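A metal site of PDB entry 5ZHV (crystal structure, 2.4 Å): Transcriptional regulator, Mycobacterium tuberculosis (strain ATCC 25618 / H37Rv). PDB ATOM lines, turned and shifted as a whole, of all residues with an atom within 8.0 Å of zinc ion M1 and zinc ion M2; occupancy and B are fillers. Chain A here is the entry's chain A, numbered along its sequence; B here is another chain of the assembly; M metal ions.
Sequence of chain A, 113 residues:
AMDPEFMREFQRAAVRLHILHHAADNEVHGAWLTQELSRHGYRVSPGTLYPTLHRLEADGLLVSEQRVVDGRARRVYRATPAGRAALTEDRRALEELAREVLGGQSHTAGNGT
The backbone carbonyl oxygen (O) of His 22 lies close to the side-chain amide oxygen (OD1) of Asn 26 (3.2 Å).
A ring nitrogen (ND1) of His 18 is in hydrogen-bond range of the backbone carbonyl oxygen (O) of Ala 14 (3.0 Å).
A ring nitrogen (ND1) of His 22 lies within hydrogen-bond range of the backbone carbonyl oxygen (O) of His 18.
NE of Arg 39 lies within salt-bridge range of OE2 of Glu 36, 2.7 Å away.
Of the 19 residues printed, 3 come within 4 Å of zinc ion M1.
Of the 19 residues printed, 3 come within 4 Å of zinc ion M2.
The nearest printed residue that does not touch zinc ion M2 is Tyr 42 (4.1 Å).
Zinc ion M1 is bound by NE2 of His 22 (2.3 Å), NE2 of His 40 (2.4 Å) and OE1 of Glu 36 (2.4 Å).
Zinc ion M1 has three donor atoms within binding distance.
Zinc ion M2 is bound by the side-chain carboxylate (OE1) of Glu 100 of chain B, the side-chain carboxylate (OE2) of Glu 100 of chain B, a ring nitrogen (NE2) of His 18 and a ring nitrogen (ND1) of His 40.
Zinc ion M2 has four donor atoms within binding distance.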
ATOM      1  N   ALA A  14     -26.143  16.894  21.577  1.00  0.00           N
ATOM      2  CA  ALA A  14     -24.749  16.622  21.220  1.00  0.00           C
ATOM      3  C   ALA A  14     -23.879  17.884  21.311  1.00  0.00           C
ATOM      4  O   ALA A  14     -22.751  17.859  21.816  1.00  0.00           O
ATOM      5  CB  ALA A  14     -24.701  16.029  19.827  1.00  0.00           C
ATOM      6  N   HIS A  18     -20.815  18.803  23.787  1.00  0.00           N
ATOM      7  CA  HIS A  18     -19.498  19.202  23.251  1.00  0.00           C
ATOM      8  C   HIS A  18     -19.029  20.526  23.798  1.00  0.00           C
ATOM      9  O   HIS A  18     -17.856  20.679  24.068  1.00  0.00           O
ATOM     10  CB  HIS A  18     -19.478  19.246  21.717  1.00  0.00           C
ATOM     11  CG  HIS A  18     -19.100  17.948  21.087  1.00  0.00           C
ATOM     12  ND1 HIS A  18     -20.027  16.957  20.827  1.00  0.00           N
ATOM     13  CD2 HIS A  18     -17.898  17.460  20.679  1.00  0.00           C
ATOM     14  CE1 HIS A  18     -19.424  15.920  20.294  1.00  0.00           C
ATOM     15  NE2 HIS A  18     -18.139  16.199  20.178  1.00  0.00           N
ATOM     16  N   HIS A  21     -17.833  19.914  27.252  1.00  0.00           N
ATOM     17  CA  HIS A  21     -16.642  19.125  27.346  1.00  0.00           C
ATOM     18  C   HIS A  21     -15.438  19.984  26.979  1.00  0.00           C
ATOM     19  O   HIS A  21     -14.442  19.952  27.687  1.00  0.00           O
ATOM     20  CB  HIS A  21     -16.705  17.811  26.588  1.00  0.00           C
ATOM     21  CG  HIS A  21     -15.390  17.077  26.610  1.00  0.00           C
ATOM     22  ND1 HIS A  21     -14.821  16.503  25.489  1.00  0.00           N
ATOM     23  CD2 HIS A  21     -14.517  16.850  27.631  1.00  0.00           C
ATOM     24  CE1 HIS A  21     -13.656  15.967  25.813  1.00  0.00           C
ATOM     25  NE2 HIS A  21     -13.445  16.162  27.101  1.00  0.00           N
ATOM     26  N   HIS A  22     -15.549  20.769  25.916  1.00  0.00           N
ATOM     27  CA  HIS A  22     -14.482  21.684  25.539  1.00  0.00           C
ATOM     28  C   HIS A  22     -14.203  22.730  26.611  1.00  0.00           C
ATOM     29  O   HIS A  22     -13.048  22.976  26.910  1.00  0.00           O
ATOM     30  CB  HIS A  22     -14.739  22.339  24.170  1.00  0.00           C
ATOM     31  CG  HIS A  22     -14.588  21.391  23.023  1.00  0.00           C
ATOM     32  ND1 HIS A  22     -15.636  20.628  22.554  1.00  0.00           N
ATOM     33  CD2 HIS A  22     -13.502  21.055  22.285  1.00  0.00           C
ATOM     34  CE1 HIS A  22     -15.209  19.873  21.551  1.00  0.00           C
ATOM     35  NE2 HIS A  22     -13.923  20.118  21.364  1.00  0.00           N
ATOM     36  N   ASP A  25     -12.183  21.259  29.598  1.00  0.00           N
ATOM     37  CA  ASP A  25     -10.787  20.979  29.261  1.00  0.00           C
ATOM     38  C   ASP A  25      -9.888  22.219  29.296  1.00  0.00           C
ATOM     39  O   ASP A  25      -8.738  22.151  29.723  1.00  0.00           O
ATOM     40  CB  ASP A  25     -10.657  20.286  27.890  1.00  0.00           C
ATOM     41  CG  ASP A  25     -10.750  18.752  27.996  1.00  0.00           C
ATOM     42  OD1 ASP A  25     -10.648  18.186  29.119  1.00  0.00           O
ATOM     43  OD2 ASP A  25     -10.945  18.088  26.939  1.00  0.00           O
ATOM     44  N   ASN A  26     -10.460  23.351  28.874  1.00  0.00           N
ATOM     45  CA  ASN A  26      -9.740  24.598  28.669  1.00  0.00           C
ATOM     46  C   ASN A  26     -10.730  25.748  28.457  1.00  0.00           C
ATOM     47  O   ASN A  26     -11.907  25.531  28.226  1.00  0.00           O
ATOM     48  CB  ASN A  26      -8.762  24.444  27.472  1.00  0.00           C
ATOM     49  CG  ASN A  26      -9.452  24.222  26.111  1.00  0.00           C
ATOM     50  OD1 ASN A  26     -10.042  23.158  25.851  1.00  0.00           O
ATOM     51  ND2 ASN A  26      -9.375  25.213  25.250  1.00  0.00           N
ATOM     52  N   TRP A  32     -13.850  30.302  18.237  1.00  0.00           N
ATOM     53  CA  TRP A  32     -13.176  29.015  18.177  1.00  0.00           C
ATOM     54  C   TRP A  32     -14.125  27.825  18.358  1.00  0.00           C
ATOM     55  O   TRP A  32     -13.990  26.812  17.663  1.00  0.00           O
ATOM     56  CB  TRP A  32     -12.064  28.945  19.185  1.00  0.00           C
ATOM     57  CG  TRP A  32     -11.260  27.683  19.085  1.00  0.00           C
ATOM     58  CD1 TRP A  32     -10.286  27.403  18.169  1.00  0.00           C
ATOM     59  CD2 TRP A  32     -11.370  26.532  19.920  1.00  0.00           C
ATOM     60  NE1 TRP A  32      -9.773  26.160  18.389  1.00  0.00           N
ATOM     61  CE2 TRP A  32     -10.411  25.590  19.461  1.00  0.00           C
ATOM     62  CE3 TRP A  32     -12.177  26.204  21.019  1.00  0.00           C
ATOM     63  CZ2 TRP A  32     -10.209  24.331  20.069  1.00  0.00           C
ATOM     64  CZ3 TRP A  32     -11.983  24.953  21.635  1.00  0.00           C
ATOM     65  CH2 TRP A  32     -11.004  24.024  21.150  1.00  0.00           C
ATOM     66  N   LEU A  33     -15.093  27.941  19.274  1.00  0.00           N
ATOM     67  CA  LEU A  33     -16.114  26.921  19.425  1.00  0.00           C
ATOM     68  C   LEU A  33     -16.827  26.621  18.120  1.00  0.00           C
ATOM     69  O   LEU A  33     -17.037  25.460  17.806  1.00  0.00           O
ATOM     70  CB  LEU A  33     -17.138  27.308  20.496  1.00  0.00           C
ATOM     71  CG  LEU A  33     -16.845  26.883  21.913  1.00  0.00           C
ATOM     72  CD1 LEU A  33     -18.020  27.267  22.789  1.00  0.00           C
ATOM     73  CD2 LEU A  33     -16.503  25.387  22.064  1.00  0.00           C
ATOM     74  N   GLN A  35     -15.684  26.940  15.029  1.00  0.00           N
ATOM     75  CA  GLN A  35     -14.741  26.128  14.236  1.00  0.00           C
ATOM     76  C   GLN A  35     -14.615  24.706  14.770  1.00  0.00           C
ATOM     77  O   GLN A  35     -14.638  23.752  14.011  1.00  0.00           O
ATOM     78  CB  GLN A  35     -13.344  26.765  14.170  1.00  0.00           C
ATOM     79  CG  GLN A  35     -13.305  28.267  13.823  1.00  0.00           C
ATOM     80  CD  GLN A  35     -13.471  28.526  12.323  1.00  0.00           C
ATOM     81  OE1 GLN A  35     -14.503  28.190  11.729  1.00  0.00           O
ATOM     82  NE2 GLN A  35     -12.424  29.107  11.687  1.00  0.00           N
ATOM     83  N   GLU A  36     -14.496  24.569  16.082  1.00  0.00           N
ATOM     84  CA  GLU A  36     -14.336  23.263  16.703  1.00  0.00           C
ATOM     85  C   GLU A  36     -15.522  22.357  16.536  1.00  0.00           C
ATOM     86  O   GLU A  36     -15.370  21.163  16.277  1.00  0.00           O
ATOM     87  CB  GLU A  36     -14.000  23.429  18.191  1.00  0.00           C
ATOM     88  CG  GLU A  36     -12.560  23.118  18.499  1.00  0.00           C
ATOM     89  CD  GLU A  36     -12.062  21.785  17.957  1.00  0.00           C
ATOM     90  OE1 GLU A  36     -12.783  20.781  18.123  1.00  0.00           O
ATOM     91  OE2 GLU A  36     -10.947  21.755  17.398  1.00  0.00           O
ATOM     92  N   LEU A  37     -16.720  22.935  16.692  1.00  0.00           N
ATOM     93  CA  LEU A  37     -17.965  22.212  16.508  1.00  0.00           C
ATOM     94  C   LEU A  37     -18.090  21.756  15.059  1.00  0.00           C
ATOM     95  O   LEU A  37     -18.444  20.600  14.804  1.00  0.00           O
ATOM     96  CB  LEU A  37     -19.155  23.039  16.950  1.00  0.00           C
ATOM     97  CG  LEU A  37     -19.265  23.194  18.482  1.00  0.00           C
ATOM     98  CD1 LEU A  37     -20.189  24.340  18.877  1.00  0.00           C
ATOM     99  CD2 LEU A  37     -19.647  21.899  19.224  1.00  0.00           C
ATOM    100  N   ARG A  39     -15.537  21.133  12.994  1.00  0.00           N
ATOM    101  CA  ARG A  39     -14.629  19.983  12.891  1.00  0.00           C
ATOM    102  C   ARG A  39     -15.280  18.681  13.368  1.00  0.00           C
ATOM    103  O   ARG A  39     -15.094  17.642  12.741  1.00  0.00           O
ATOM    104  CB  ARG A  39     -13.314  20.219  13.649  1.00  0.00           C
ATOM    105  CG  ARG A  39     -12.240  20.964  12.887  1.00  0.00           C
ATOM    106  CD  ARG A  39     -10.924  21.051  13.684  1.00  0.00           C
ATOM    107  NE  ARG A  39     -10.987  22.049  14.755  1.00  0.00           N
ATOM    108  CZ  ARG A  39     -10.650  23.342  14.644  1.00  0.00           C
ATOM    109  NH1 ARG A  39     -10.200  23.824  13.482  1.00  0.00           N
ATOM    110  NH2 ARG A  39     -10.755  24.160  15.696  1.00  0.00           N
ATOM    111  N   HIS A  40     -16.061  18.749  14.444  1.00  0.00           N
ATOM    112  CA  HIS A  40     -16.724  17.561  14.971  1.00  0.00           C
ATOM    113  C   HIS A  40     -17.983  17.171  14.180  1.00  0.00           C
ATOM    114  O   HIS A  40     -18.642  16.200  14.528  1.00  0.00           O
ATOM    115  CB  HIS A  40     -17.052  17.751  16.450  1.00  0.00           C
ATOM    116  CG  HIS A  40     -15.874  17.620  17.367  1.00  0.00           C
ATOM    117  ND1 HIS A  40     -15.310  16.406  17.696  1.00  0.00           N
ATOM    118  CD2 HIS A  40     -15.192  18.553  18.074  1.00  0.00           C
ATOM    119  CE1 HIS A  40     -14.316  16.598  18.546  1.00  0.00           C
ATOM    120  NE2 HIS A  40     -14.221  17.890  18.803  1.00  0.00           N
ATOM    121  N   GLY A  41     -18.309  17.939  13.145  1.00  0.00           N
ATOM    122  CA  GLY A  41     -19.423  17.631  12.256  1.00  0.00           C
ATOM    123  C   GLY A  41     -20.779  18.234  12.611  1.00  0.00           C
ATOM    124  O   GLY A  41     -21.813  17.665  12.267  1.00  0.00           O
ATOM    125  N   TYR A  42     -20.797  19.378  13.284  1.00  0.00           N
ATOM    126  CA  TYR A  42     -22.061  20.030  13.633  1.00  0.00           C
ATOM    127  C   TYR A  42     -22.159  21.394  12.971  1.00  0.00           C
ATOM    128  O   TYR A  42     -21.261  22.242  13.104  1.00  0.00           O
ATOM    129  CB  TYR A  42     -22.263  20.094  15.151  1.00  0.00           C
ATOM    130  CG  TYR A  42     -22.176  18.737  15.841  1.00  0.00           C
ATOM    131  CD1 TYR A  42     -23.276  17.846  15.880  1.00  0.00           C
ATOM    132  CD2 TYR A  42     -20.981  18.320  16.424  1.00  0.00           C
ATOM    133  CE1 TYR A  42     -23.172  16.588  16.513  1.00  0.00           C
ATOM    134  CE2 TYR A  42     -20.876  17.076  17.058  1.00  0.00           C
ATOM    135  CZ  TYR A  42     -21.949  16.219  17.080  1.00  0.00           C
ATOM    136  OH  TYR A  42     -21.773  15.005  17.695  1.00  0.00           O
ATOM    137  N   GLU B  96     -21.810   6.652  17.665  1.00  0.00           N
ATOM    138  CA  GLU B  96     -20.697   7.533  17.346  1.00  0.00           C
ATOM    139  C   GLU B  96     -20.388   8.410  18.542  1.00  0.00           C
ATOM    140  O   GLU B  96     -19.246   8.405  19.009  1.00  0.00           O
ATOM    141  CB  GLU B  96     -20.979   8.379  16.116  1.00  0.00           C
ATOM    142  CG  GLU B  96     -20.741   7.640  14.801  1.00  0.00           C
ATOM    143  CD  GLU B  96     -20.830   8.554  13.571  1.00  0.00           C
ATOM    144  OE1 GLU B  96     -20.100   9.577  13.497  1.00  0.00           O
ATOM    145  OE2 GLU B  96     -21.618   8.225  12.649  1.00  0.00           O
ATOM    146  N   LEU B  97     -21.430   9.095  19.057  1.00  0.00           N
ATOM    147  CA  LEU B  97     -21.263  10.015  20.172  1.00  0.00           C
ATOM    148  C   LEU B  97     -20.846   9.312  21.453  1.00  0.00           C
ATOM    149  O   LEU B  97     -20.008   9.832  22.212  1.00  0.00           O
ATOM    150  CB  LEU B  97     -22.526  10.847  20.391  1.00  0.00           C
ATOM    151  CG  LEU B  97     -22.414  11.958  21.418  1.00  0.00           C
ATOM    152  CD1 LEU B  97     -21.347  12.959  21.001  1.00  0.00           C
ATOM    153  CD2 LEU B  97     -23.748  12.662  21.595  1.00  0.00           C
ATOM    154  N   GLU B 100     -17.125   8.442  21.152  1.00  0.00           N
ATOM    155  CA  GLU B 100     -16.306   9.652  21.266  1.00  0.00           C
ATOM    156  C   GLU B 100     -16.058  10.118  22.713  1.00  0.00           C
ATOM    157  O   GLU B 100     -14.922  10.457  23.050  1.00  0.00           O
ATOM    158  CB  GLU B 100     -16.957  10.763  20.457  1.00  0.00           C
ATOM    159  CG  GLU B 100     -16.148  12.037  20.297  1.00  0.00           C
ATOM    160  CD  GLU B 100     -16.980  13.167  19.693  1.00  0.00           C
ATOM    161  OE1 GLU B 100     -16.430  14.279  19.533  1.00  0.00           O
ATOM    162  OE2 GLU B 100     -18.175  12.975  19.359  1.00  0.00           O
ATOM    163  N   VAL B 101     -17.089  10.120  23.548  1.00  0.00           N
ATOM    164  CA  VAL B 101     -16.966  10.706  24.896  1.00  0.00           C
ATOM    165  C   VAL B 101     -16.800   9.729  26.057  1.00  0.00           C
ATOM    166  O   VAL B 101     -16.541  10.152  27.161  1.00  0.00           O
ATOM    167  CB  VAL B 101     -18.061  11.777  25.193  1.00  0.00           C
ATOM    168  CG1 VAL B 101     -18.010  12.895  24.157  1.00  0.00           C
ATOM    169  CG2 VAL B 101     -19.445  11.152  25.271  1.00  0.00           C
HETATM  170 ZN    ZN M   1     -12.499  19.114  19.884  1.00  0.00          ZN
HETATM  171 ZN    ZN M   2     -17.554  14.992  18.093  1.00  0.00          ZN
HETATM  172 ZN    ZN M   3     -16.138  15.609  24.250  1.00  0.00          ZN
